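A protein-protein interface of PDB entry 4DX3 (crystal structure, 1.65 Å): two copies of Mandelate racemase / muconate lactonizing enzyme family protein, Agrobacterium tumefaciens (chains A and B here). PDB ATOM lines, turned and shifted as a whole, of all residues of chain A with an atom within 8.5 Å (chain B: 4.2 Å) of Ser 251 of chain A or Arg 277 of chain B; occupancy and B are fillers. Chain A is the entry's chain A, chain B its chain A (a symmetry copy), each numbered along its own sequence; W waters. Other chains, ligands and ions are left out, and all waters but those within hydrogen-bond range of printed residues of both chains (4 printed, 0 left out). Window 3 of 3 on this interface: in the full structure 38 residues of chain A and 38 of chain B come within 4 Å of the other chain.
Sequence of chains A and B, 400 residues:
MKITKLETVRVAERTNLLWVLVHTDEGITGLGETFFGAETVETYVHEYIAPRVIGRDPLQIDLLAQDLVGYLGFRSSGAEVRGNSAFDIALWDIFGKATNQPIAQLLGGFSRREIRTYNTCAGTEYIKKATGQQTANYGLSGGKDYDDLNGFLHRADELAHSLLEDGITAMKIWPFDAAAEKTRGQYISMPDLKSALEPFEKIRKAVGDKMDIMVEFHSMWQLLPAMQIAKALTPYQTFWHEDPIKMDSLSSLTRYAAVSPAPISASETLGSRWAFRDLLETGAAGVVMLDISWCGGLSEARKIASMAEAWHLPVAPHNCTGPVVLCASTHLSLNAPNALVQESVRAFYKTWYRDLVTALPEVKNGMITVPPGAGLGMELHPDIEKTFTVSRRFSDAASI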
ATOM      1  N   ARG A  75     -30.302  10.469  -5.520  1.00  0.00           N
ATOM      2  CA  ARG A  75     -29.619  10.340  -6.813  1.00  0.00           C
ATOM      3  C   ARG A  75     -28.382   9.446  -6.676  1.00  0.00           C
ATOM      4  O   ARG A  75     -27.263   9.798  -7.093  1.00  0.00           O
ATOM      5  CB  ARG A  75     -29.236  11.724  -7.352  1.00  0.00           C
ATOM      6  CG  ARG A  75     -28.789  11.721  -8.818  1.00  0.00           C
ATOM      7  CD  ARG A  75     -27.561  12.612  -8.949  1.00  0.00           C
ATOM      8  NE  ARG A  75     -27.062  12.718 -10.324  1.00  0.00           N
ATOM      9  CZ  ARG A  75     -26.063  11.986 -10.814  1.00  0.00           C
ATOM     10  NH1 ARG A  75     -25.459  11.081 -10.054  1.00  0.00           N
ATOM     11  NH2 ARG A  75     -25.672  12.161 -12.074  1.00  0.00           N
ATOM     12  N   LEU A 223     -10.068   6.636 -17.393  1.00  0.00           N
ATOM     13  CA  LEU A 223     -10.494   6.981 -18.749  1.00  0.00           C
ATOM     14  C   LEU A 223      -9.530   6.508 -19.822  1.00  0.00           C
ATOM     15  O   LEU A 223      -9.951   5.910 -20.812  1.00  0.00           O
ATOM     16  CB  LEU A 223     -10.722   8.496 -18.892  1.00  0.00           C
ATOM     17  CG  LEU A 223     -11.139   8.932 -20.301  1.00  0.00           C
ATOM     18  CD1 LEU A 223     -12.484   8.334 -20.704  1.00  0.00           C
ATOM     19  CD2 LEU A 223     -11.175  10.446 -20.402  1.00  0.00           C
ATOM     20  N   ILE A 245     -16.034   3.085 -17.229  1.00  0.00           N
ATOM     21  CA  ILE A 245     -15.402   3.897 -16.194  1.00  0.00           C
ATOM     22  C   ILE A 245     -16.394   4.096 -15.054  1.00  0.00           C
ATOM     23  O   ILE A 245     -17.558   3.706 -15.170  1.00  0.00           O
ATOM     24  CB  ILE A 245     -14.963   5.280 -16.721  1.00  0.00           C
ATOM     25  CG1 ILE A 245     -16.174   6.081 -17.215  1.00  0.00           C
ATOM     26  CG2 ILE A 245     -13.886   5.131 -17.812  1.00  0.00           C
ATOM     27  CD1 ILE A 245     -15.821   7.528 -17.601  1.00  0.00           C
ATOM     28  N   LYS A 246     -15.930   4.685 -13.951  1.00  0.00           N
ATOM     29  CA  LYS A 246     -16.828   5.011 -12.838  1.00  0.00           C
ATOM     30  C   LYS A 246     -17.892   6.009 -13.303  1.00  0.00           C
ATOM     31  O   LYS A 246     -17.590   6.965 -14.025  1.00  0.00           O
ATOM     32  CB  LYS A 246     -16.027   5.606 -11.670  1.00  0.00           C
ATOM     33  CG  LYS A 246     -16.756   5.621 -10.309  1.00  0.00           C
ATOM     34  CD  LYS A 246     -16.776   4.247  -9.686  1.00  0.00           C
ATOM     35  CE  LYS A 246     -17.280   4.283  -8.242  1.00  0.00           C
ATOM     36  NZ  LYS A 246     -17.290   2.894  -7.695  1.00  0.00           N
ATOM     37  N   MET A 247     -19.132   5.815 -12.864  1.00  0.00           N
ATOM     38  CA  MET A 247     -20.231   6.665 -13.328  1.00  0.00           C
ATOM     39  C   MET A 247     -20.474   7.844 -12.401  1.00  0.00           C
ATOM     40  O   MET A 247     -21.621   8.153 -12.068  1.00  0.00           O
ATOM     41  CB  MET A 247     -21.508   5.832 -13.496  1.00  0.00           C
ATOM     42  CG  MET A 247     -21.388   4.769 -14.581  1.00  0.00           C
ATOM     43  SD  MET A 247     -21.381   5.534 -16.214  1.00  0.00           S
ATOM     44  CE  MET A 247     -20.591   4.248 -17.203  1.00  0.00           C
ATOM     45  N   ASP A 248     -19.398   8.527 -12.006  1.00  0.00           N
ATOM     46  CA  ASP A 248     -19.531   9.632 -11.058  1.00  0.00           C
ATOM     47  C   ASP A 248     -19.439  11.051 -11.638  1.00  0.00           C
ATOM     48  O   ASP A 248     -19.917  12.002 -11.028  1.00  0.00           O
ATOM     49  CB  ASP A 248     -18.569   9.468  -9.877  1.00  0.00           C
ATOM     50  CG  ASP A 248     -17.146   9.189 -10.303  1.00  0.00           C
ATOM     51  OD1 ASP A 248     -16.828   9.202 -11.515  1.00  0.00           O
ATOM     52  OD2 ASP A 248     -16.331   8.956  -9.391  1.00  0.00           O
ATOM     53  N   SER A 249     -18.814  11.193 -12.795  1.00  0.00           N
ATOM     54  CA  SER A 249     -18.838  12.458 -13.533  1.00  0.00           C
ATOM     55  C   SER A 249     -19.139  12.050 -14.961  1.00  0.00           C
ATOM     56  O   SER A 249     -18.247  11.671 -15.716  1.00  0.00           O
ATOM     57  CB  SER A 249     -17.493  13.201 -13.458  1.00  0.00           C
ATOM     58  OG  SER A 249     -17.325  13.904 -12.232  1.00  0.00           O
ATOM     59  N   LEU A 250     -20.413  12.093 -15.323  1.00  0.00           N
ATOM     60  CA  LEU A 250     -20.838  11.454 -16.560  1.00  0.00           C
ATOM     61  C   LEU A 250     -20.333  12.153 -17.824  1.00  0.00           C
ATOM     62  O   LEU A 250     -20.312  11.546 -18.898  1.00  0.00           O
ATOM     63  CB  LEU A 250     -22.363  11.342 -16.580  1.00  0.00           C
ATOM     64  CG  LEU A 250     -22.931  10.467 -15.463  1.00  0.00           C
ATOM     65  CD1 LEU A 250     -24.451  10.550 -15.418  1.00  0.00           C
ATOM     66  CD2 LEU A 250     -22.470   9.016 -15.602  1.00  0.00           C
ATOM     67  N   SER A 251     -19.930  13.414 -17.715  1.00  0.00           N
ATOM     68  CA  SER A 251     -19.433  14.119 -18.894  1.00  0.00           C
ATOM     69  C   SER A 251     -18.199  13.439 -19.490  1.00  0.00           C
ATOM     70  O   SER A 251     -17.925  13.571 -20.684  1.00  0.00           O
ATOM     71  CB  SER A 251     -19.143  15.595 -18.586  1.00  0.00           C
ATOM     72  OG  SER A 251     -18.087  15.741 -17.660  1.00  0.00           O
ATOM     73  N   SER A 252     -17.460  12.701 -18.666  1.00  0.00           N
ATOM     74  CA  SER A 252     -16.298  11.959 -19.164  1.00  0.00           C
ATOM     75  C   SER A 252     -16.670  10.909 -20.217  1.00  0.00           C
ATOM     76  O   SER A 252     -15.827  10.507 -21.012  1.00  0.00           O
ATOM     77  CB  SER A 252     -15.533  11.310 -18.010  1.00  0.00           C
ATOM     78  OG  SER A 252     -14.844  12.288 -17.248  1.00  0.00           O
ATOM     79  N   LEU A 253     -17.934  10.483 -20.237  1.00  0.00           N
ATOM     80  CA  LEU A 253     -18.365   9.477 -21.205  1.00  0.00           C
ATOM     81  C   LEU A 253     -18.268   9.956 -22.648  1.00  0.00           C
ATOM     82  O   LEU A 253     -18.165   9.133 -23.552  1.00  0.00           O
ATOM     83  CB  LEU A 253     -19.794   8.988 -20.911  1.00  0.00           C
ATOM     84  CG  LEU A 253     -19.944   8.246 -19.592  1.00  0.00           C
ATOM     85  CD1 LEU A 253     -21.407   7.898 -19.348  1.00  0.00           C
ATOM     86  CD2 LEU A 253     -19.081   6.990 -19.571  1.00  0.00           C
ATOM     87  N   THR A 254     -18.305  11.266 -22.881  1.00  0.00           N
ATOM     88  CA  THR A 254     -18.152  11.754 -24.257  1.00  0.00           C
ATOM     89  C   THR A 254     -16.780  11.384 -24.831  1.00  0.00           C
ATOM     90  O   THR A 254     -16.672  11.064 -26.021  1.00  0.00           O
ATOM     91  CB  THR A 254     -18.387  13.275 -24.387  1.00  0.00           C
ATOM     92  OG1 THR A 254     -17.330  13.987 -23.735  1.00  0.00           O
ATOM     93  CG2 THR A 254     -19.728  13.650 -23.767  1.00  0.00           C
ATOM     94  N   ARG A 255     -15.748  11.408 -23.985  1.00  0.00           N
ATOM     95  CA  ARG A 255     -14.390  11.035 -24.415  1.00  0.00           C
ATOM     96  C   ARG A 255     -14.382   9.573 -24.853  1.00  0.00           C
ATOM     97  O   ARG A 255     -13.764   9.204 -25.853  1.00  0.00           O
ATOM     98  CB  ARG A 255     -13.387  11.198 -23.266  1.00  0.00           C
ATOM     99  CG  ARG A 255     -13.235  12.614 -22.682  1.00  0.00           C
ATOM    100  CD  ARG A 255     -12.488  13.524 -23.616  1.00  0.00           C
ATOM    101  NE  ARG A 255     -11.158  13.016 -23.970  1.00  0.00           N
ATOM    102  CZ  ARG A 255     -10.043  13.226 -23.263  1.00  0.00           C
ATOM    103  NH1 ARG A 255     -10.077  13.928 -22.136  1.00  0.00           N
ATOM    104  NH2 ARG A 255      -8.886  12.731 -23.693  1.00  0.00           N
ATOM    105  N   TYR A 256     -15.091   8.742 -24.100  1.00  0.00           N
ATOM    106  CA  TYR A 256     -15.122   7.309 -24.374  1.00  0.00           C
ATOM    107  C   TYR A 256     -15.919   6.996 -25.637  1.00  0.00           C
ATOM    108  O   TYR A 256     -15.504   6.178 -26.457  1.00  0.00           O
ATOM    109  CB  TYR A 256     -15.724   6.575 -23.175  1.00  0.00           C
ATOM    110  CG  TYR A 256     -15.654   5.071 -23.301  1.00  0.00           C
ATOM    111  CD1 TYR A 256     -14.504   4.376 -22.931  1.00  0.00           C
ATOM    112  CD2 TYR A 256     -16.737   4.350 -23.785  1.00  0.00           C
ATOM    113  CE1 TYR A 256     -14.435   2.999 -23.046  1.00  0.00           C
ATOM    114  CE2 TYR A 256     -16.677   2.981 -23.912  1.00  0.00           C
ATOM    115  CZ  TYR A 256     -15.527   2.312 -23.540  1.00  0.00           C
ATOM    116  OH  TYR A 256     -15.469   0.949 -23.648  1.00  0.00           O
ATOM    117  N   ALA A 257     -17.076   7.637 -25.781  1.00  0.00           N
ATOM    118  CA  ALA A 257     -17.931   7.401 -26.943  1.00  0.00           C
ATOM    119  C   ALA A 257     -17.238   7.774 -28.248  1.00  0.00           C
ATOM    120  O   ALA A 257     -17.547   7.203 -29.299  1.00  0.00           O
ATOM    121  CB  ALA A 257     -19.248   8.168 -26.807  1.00  0.00           C
ATOM    122  N   ILE A 264     -22.081   2.573 -25.325  1.00  0.00           N
ATOM    123  CA  ILE A 264     -21.903   2.515 -23.886  1.00  0.00           C
ATOM    124  C   ILE A 264     -23.166   1.958 -23.261  1.00  0.00           C
ATOM    125  O   ILE A 264     -24.271   2.398 -23.559  1.00  0.00           O
ATOM    126  CB  ILE A 264     -21.641   3.917 -23.308  1.00  0.00           C
ATOM    127  CG1 ILE A 264     -20.308   4.467 -23.837  1.00  0.00           C
ATOM    128  CG2 ILE A 264     -21.639   3.880 -21.784  1.00  0.00           C
ATOM    129  CD1 ILE A 264     -20.098   5.962 -23.522  1.00  0.00           C
ATOM    130  N   ASP A 278     -29.095  13.155 -16.526  1.00  0.00           N
ATOM    131  CA  ASP A 278     -27.702  13.570 -16.708  1.00  0.00           C
ATOM    132  C   ASP A 278     -26.987  12.703 -17.751  1.00  0.00           C
ATOM    133  O   ASP A 278     -26.243  13.228 -18.579  1.00  0.00           O
ATOM    134  CB  ASP A 278     -26.915  13.527 -15.392  1.00  0.00           C
ATOM    135  CG  ASP A 278     -27.411  14.534 -14.362  1.00  0.00           C
ATOM    136  OD1 ASP A 278     -28.181  15.463 -14.707  1.00  0.00           O
ATOM    137  OD2 ASP A 278     -27.008  14.402 -13.183  1.00  0.00           O
ATOM    138  N   LEU A 279     -27.205  11.383 -17.703  1.00  0.00           N
ATOM    139  CA  LEU A 279     -26.594  10.475 -18.666  1.00  0.00           C
ATOM    140  C   LEU A 279     -27.068  10.797 -20.085  1.00  0.00           C
ATOM    141  O   LEU A 279     -26.260  10.909 -21.014  1.00  0.00           O
ATOM    142  CB  LEU A 279     -26.946   9.033 -18.291  1.00  0.00           C
ATOM    143  CG  LEU A 279     -26.523   7.959 -19.298  1.00  0.00           C
ATOM    144  CD1 LEU A 279     -25.005   7.879 -19.409  1.00  0.00           C
ATOM    145  CD2 LEU A 279     -27.112   6.604 -18.903  1.00  0.00           C
ATOM    146  N   GLU A 281     -28.230  13.559 -21.284  1.00  0.00           N
ATOM    147  CA  GLU A 281     -27.792  14.881 -21.726  1.00  0.00           C
ATOM    148  C   GLU A 281     -26.320  14.944 -22.133  1.00  0.00           C
ATOM    149  O   GLU A 281     -25.894  15.938 -22.734  1.00  0.00           O
ATOM    150  CB  GLU A 281     -28.107  15.948 -20.669  1.00  0.00           C
ATOM    151  CG  GLU A 281     -29.596  16.242 -20.536  1.00  0.00           C
ATOM    152  CD  GLU A 281     -29.894  17.426 -19.611  1.00  0.00           C
ATOM    153  OE1 GLU A 281     -29.229  17.552 -18.559  1.00  0.00           O
ATOM    154  OE2 GLU A 281     -30.790  18.228 -19.943  1.00  0.00           O
ATOM    155  N   THR A 282     -25.545  13.902 -21.821  1.00  0.00           N
ATOM    156  CA  THR A 282     -24.150  13.864 -22.271  1.00  0.00           C
ATOM    157  C   THR A 282     -24.059  13.744 -23.777  1.00  0.00           C
ATOM    158  O   THR A 282     -23.048  14.129 -24.376  1.00  0.00           O
ATOM    159  CB  THR A 282     -23.345  12.680 -21.702  1.00  0.00           C
ATOM    160  OG1 THR A 282     -23.883  11.440 -22.182  1.00  0.00           O
ATOM    161  CG2 THR A 282     -23.344  12.696 -20.184  1.00  0.00           C
ATOM    162  N   GLY A 283     -25.100  13.186 -24.384  1.00  0.00           N
ATOM    163  CA  GLY A 283     -25.057  12.859 -25.798  1.00  0.00           C
ATOM    164  C   GLY A 283     -24.232  11.619 -26.109  1.00  0.00           C
ATOM    165  O   GLY A 283     -23.940  11.352 -27.272  1.00  0.00           O
ATOM    166  N   ALA A 284     -23.847  10.869 -25.076  1.00  0.00           N
ATOM    167  CA  ALA A 284     -23.050   9.650 -25.234  1.00  0.00           C
ATOM    168  C   ALA A 284     -23.785   8.397 -24.778  1.00  0.00           C
ATOM    169  O   ALA A 284     -23.216   7.300 -24.782  1.00  0.00           O
ATOM    170  CB  ALA A 284     -21.734   9.777 -24.469  1.00  0.00           C
ATOM    171  N   ARG B 273     -15.346  14.593  -4.724  1.00  0.00           N
ATOM    172  CA  ARG B 273     -14.862  15.662  -5.577  1.00  0.00           C
ATOM    173  C   ARG B 273     -15.480  15.592  -6.964  1.00  0.00           C
ATOM    174  O   ARG B 273     -15.510  16.594  -7.677  1.00  0.00           O
ATOM    175  CB  ARG B 273     -13.334  15.655  -5.634  1.00  0.00           C
ATOM    176  CG  ARG B 273     -12.744  14.723  -6.618  1.00  0.00           C
ATOM    177  CD  ARG B 273     -11.250  14.632  -6.329  1.00  0.00           C
ATOM    178  NE  ARG B 273     -11.007  13.650  -5.280  1.00  0.00           N
ATOM    179  CZ  ARG B 273      -9.899  12.931  -5.203  1.00  0.00           C
ATOM    180  NH1 ARG B 273      -8.928  13.146  -6.080  1.00  0.00           N
ATOM    181  NH2 ARG B 273      -9.751  12.019  -4.249  1.00  0.00           N
ATOM    182  N   TRP B 274     -15.996  14.421  -7.335  1.00  0.00           N
ATOM    183  CA  TRP B 274     -16.653  14.258  -8.638  1.00  0.00           C
ATOM    184  C   TRP B 274     -17.972  15.015  -8.755  1.00  0.00           C
ATOM    185  O   TRP B 274     -18.294  15.573  -9.818  1.00  0.00           O
ATOM    186  CB  TRP B 274     -16.804  12.764  -8.999  1.00  0.00           C
ATOM    187  CG  TRP B 274     -15.462  12.154  -9.276  1.00  0.00           C
ATOM    188  CD1 TRP B 274     -14.847  12.055 -10.489  1.00  0.00           C
ATOM    189  CD2 TRP B 274     -14.537  11.631  -8.314  1.00  0.00           C
ATOM    190  NE1 TRP B 274     -13.611  11.470 -10.349  1.00  0.00           N
ATOM    191  CE2 TRP B 274     -13.391  11.214  -9.022  1.00  0.00           C
ATOM    192  CE3 TRP B 274     -14.561  11.473  -6.924  1.00  0.00           C
ATOM    193  CZ2 TRP B 274     -12.285  10.636  -8.387  1.00  0.00           C
ATOM    194  CZ3 TRP B 274     -13.464  10.900  -6.297  1.00  0.00           C
ATOM    195  CH2 TRP B 274     -12.342  10.488  -7.029  1.00  0.00           C
ATOM    196  N   ALA B 275     -18.743  15.039  -7.678  1.00  0.00           N
ATOM    197  CA  ALA B 275     -19.957  15.847  -7.670  1.00  0.00           C
ATOM    198  C   ALA B 275     -19.582  17.324  -7.774  1.00  0.00           C
ATOM    199  O   ALA B 275     -20.286  18.110  -8.405  1.00  0.00           O
ATOM    200  CB  ALA B 275     -20.758  15.594  -6.408  1.00  0.00           C
ATOM    201  N   PHE B 276     -18.480  17.703  -7.138  1.00  0.00           N
ATOM    202  CA  PHE B 276     -18.061  19.100  -7.173  1.00  0.00           C
ATOM    203  C   PHE B 276     -17.435  19.493  -8.502  1.00  0.00           C
ATOM    204  O   PHE B 276     -17.573  20.645  -8.921  1.00  0.00           O
ATOM    205  CB  PHE B 276     -17.210  19.454  -5.953  1.00  0.00           C
ATOM    206  CG  PHE B 276     -18.026  19.551  -4.707  1.00  0.00           C
ATOM    207  CD1 PHE B 276     -18.632  20.747  -4.355  1.00  0.00           C
ATOM    208  CD2 PHE B 276     -18.253  18.427  -3.924  1.00  0.00           C
ATOM    209  CE1 PHE B 276     -19.422  20.829  -3.207  1.00  0.00           C
ATOM    210  CE2 PHE B 276     -19.043  18.503  -2.778  1.00  0.00           C
ATOM    211  CZ  PHE B 276     -19.617  19.700  -2.419  1.00  0.00           C
ATOM    212  N   ARG B 277     -16.784  18.542  -9.178  1.00  0.00           N
ATOM    213  CA  ARG B 277     -16.390  18.776 -10.568  1.00  0.00           C
ATOM    214  C   ARG B 277     -17.636  19.076 -11.393  1.00  0.00           C
ATOM    215  O   ARG B 277     -17.668  20.053 -12.153  1.00  0.00           O
ATOM    216  CB  ARG B 277     -15.624  17.586 -11.160  1.00  0.00           C
ATOM    217  CG  ARG B 277     -15.617  17.597 -12.688  1.00  0.00           C
ATOM    218  CD  ARG B 277     -14.848  16.425 -13.290  1.00  0.00           C
ATOM    219  NE  ARG B 277     -15.153  16.330 -14.722  1.00  0.00           N
ATOM    220  CZ  ARG B 277     -15.079  15.227 -15.462  1.00  0.00           C
ATOM    221  NH1 ARG B 277     -14.645  14.075 -14.953  1.00  0.00           N
ATOM    222  NH2 ARG B 277     -15.410  15.299 -16.743  1.00  0.00           N
ATOM    223  N   ASP B 278     -18.677  18.257 -11.239  1.00  0.00           N
ATOM    224  CA  ASP B 278     -19.912  18.488 -11.992  1.00  0.00           C
ATOM    225  C   ASP B 278     -20.500  19.872 -11.699  1.00  0.00           C
ATOM    226  O   ASP B 278     -20.948  20.556 -12.619  1.00  0.00           O
ATOM    227  CB  ASP B 278     -20.971  17.418 -11.698  1.00  0.00           C
ATOM    228  CG  ASP B 278     -20.568  16.027 -12.174  1.00  0.00           C
ATOM    229  OD1 ASP B 278     -19.606  15.885 -12.967  1.00  0.00           O
ATOM    230  OD2 ASP B 278     -21.242  15.056 -11.757  1.00  0.00           O
ATOM    231  N   LEU B 279     -20.506  20.278 -10.423  1.00  0.00           N
ATOM    232  CA  LEU B 279     -21.019  21.587 -10.041  1.00  0.00           C
ATOM    233  C   LEU B 279     -20.195  22.699 -10.696  1.00  0.00           C
ATOM    234  O   LEU B 279     -20.746  23.636 -11.284  1.00  0.00           O
ATOM    235  CB  LEU B 279     -20.987  21.716  -8.516  1.00  0.00           C
ATOM    236  CG  LEU B 279     -21.335  23.098  -7.955  1.00  0.00           C
ATOM    237  CD1 LEU B 279     -22.783  23.465  -8.259  1.00  0.00           C
ATOM    238  CD2 LEU B 279     -21.067  23.140  -6.450  1.00  0.00           C
ATOM    239  N   LEU B 280     -18.874  22.579 -10.626  1.00  0.00           N
ATOM    240  CA  LEU B 280     -18.001  23.624 -11.185  1.00  0.00           C
ATOM    241  C   LEU B 280     -18.174  23.742 -12.701  1.00  0.00           C
ATOM    242  O   LEU B 280     -18.134  24.845 -13.265  1.00  0.00           O
ATOM    243  CB  LEU B 280     -16.535  23.330 -10.846  1.00  0.00           C
ATOM    244  CG  LEU B 280     -16.189  23.521  -9.373  1.00  0.00           C
ATOM    245  CD1 LEU B 280     -14.761  23.022  -9.100  1.00  0.00           C
ATOM    246  CD2 LEU B 280     -16.343  24.985  -8.936  1.00  0.00           C
ATOM    247  N   GLU B 281     -18.379  22.609 -13.363  1.00  0.00           N
ATOM    248  CA  GLU B 281     -18.496  22.600 -14.820  1.00  0.00           C
ATOM    249  C   GLU B 281     -19.812  23.178 -15.341  1.00  0.00           C
ATOM    250  O   GLU B 281     -19.933  23.433 -16.545  1.00  0.00           O
ATOM    251  CB  GLU B 281     -18.265  21.191 -15.382  1.00  0.00           C
ATOM    252  CG  GLU B 281     -16.816  20.731 -15.274  1.00  0.00           C
ATOM    253  CD  GLU B 281     -16.554  19.402 -15.990  1.00  0.00           C
ATOM    254  OE1 GLU B 281     -17.410  18.494 -15.910  1.00  0.00           O
ATOM    255  OE2 GLU B 281     -15.493  19.275 -16.635  1.00  0.00           O
HETATM  256  O   HOH W   1     -20.396  17.983 -16.306  1.00  0.00           O
HETATM  257  O   HOH W   2     -22.281  13.210 -13.406  1.00  0.00           O
HETATM  258  O   HOH W   3     -20.533  15.371 -15.545  1.00  0.00           O
HETATM  259  O   HOH W   4     -15.358  15.456 -19.838  1.00  0.00           O
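Among the printed residues, pairs that only touch across the chains: Asp 248 of chain A with Trp 274 of chain B (3.3 Å) and Ser 249 of chain A with Arg 277 of chain B (3.3 Å).
Water W2 lies within hydrogen-bond range of the side-chain carboxylate of Asp 278 of chain B (2.7 Å) and the backbone NH of Leu 250 of chain A (2.9 Å). Water W3 lies within hydrogen-bond range of the side-chain carboxylate of Asp 278 of chain B (2.8 Å), the backbone NH of Ser 251 of chain A (3.0 Å) and the backbone NH of Leu 250 of chain A (3.3 Å). Water W1 bridges the side-chain carboxylate of Glu 281 of chain B (3.1 Å) and the side-chain hydroxyl of Ser 251 of chain A (3.5 Å). Water W4 lies within hydrogen-bond range of NH2 of Arg 277 of chain B (3.1 Å) and O of Ser 251 of chain A (3.3 Å).
3 positions are printed for both chains. Of the 8 pairs that touch across the chains among the printed residues, none has its exchanged pair printed and touching as well.
Of the 9 printed residues of chain B, 4 touch a printed residue of chain A. Hydrophobic or aromatic side chains of chain B within 4 Å of the printed part of chain A: Trp 274. Printed residues of chain A that touch a printed residue of chain B: Asp 248, Ser 249, Ser 251 and Ser 252. Among the printed residues, no Asp or Glu carboxylate lies within 4 Å of a Lys or Arg side-chain nitrogen of the other chain.
The side-chain hydroxyl (OG) of Ser 249 of chain A is in hydrogen-bond range of the backbone carbonyl oxygen (O) of Trp 274 of chain B (3.1 Å). OD1 of Asp 278 of chain B sits at hydrogen-bond distance from OG of Ser 249 of chain A (3.1 Å). The guanidinium group (NH2) of Arg 277 of chain B lies within hydrogen-bond range of the side-chain hydroxyl (OG) of Ser 251 of chain A. OG of Ser 251 of chain A is in hydrogen-bond range of OE1 of Glu 281 of chain B, 3.3 Å away. The guanidinium group (NH1) of Arg 277 of chain B lies within hydrogen-bond range of the side-chain hydroxyl (OG) of Ser 252 of chain A (2.9 Å). O of Asp 248 of chain A sits close to OD2 of Asp 278 of chain B, at 3.4 Å.
Of the printed residues of chain B, Ser 251 of chain A touches Arg 277 (2.9 Å) and Glu 281 (3.3 Å). Printed residues of chain A within 4 Å of Arg 277 of chain B: Ser 249 (3.3 Å), Ser 251 (2.9 Å) and Ser 252 (2.9 Å). Of the printed residues of chain B, Ser 249 of chain A touches Trp 274 (3.1 Å), Arg 277 (3.3 Å) and Asp 278 (3.1 Å). Of the printed residues of chain A, Asp 278 of chain B touches Asp 248 (3.4 Å) and Ser 249 (3.1 Å). Of the printed residues of chain A, Glu 281 of chain B touches Ser 251. Of the printed residues of chain A, Trp 274 of chain B touches Asp 248 and Ser 249. Ala 284 of chain A touches none of the printed residues of chain B. Lys 246 of chain A touches none of the printed residues of chain B. The nearest printed residue of chain B that does not touch Ser 251 of chain A is Asp 278 of chain B (4.9 Å). The nearest printed residue of chain A that does not touch Arg 277 of chain B is Leu 250 of chain A (5.9 Å).
O of Ser 251 of chain A is in hydrogen-bond range of OG1 of Thr 254 of chain A, at 3.1 Å. The guanidinium group (NE) of Arg 277 of chain B is in salt-bridge range of the side-chain carboxylate (OE1) of Glu 281 of chain B.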
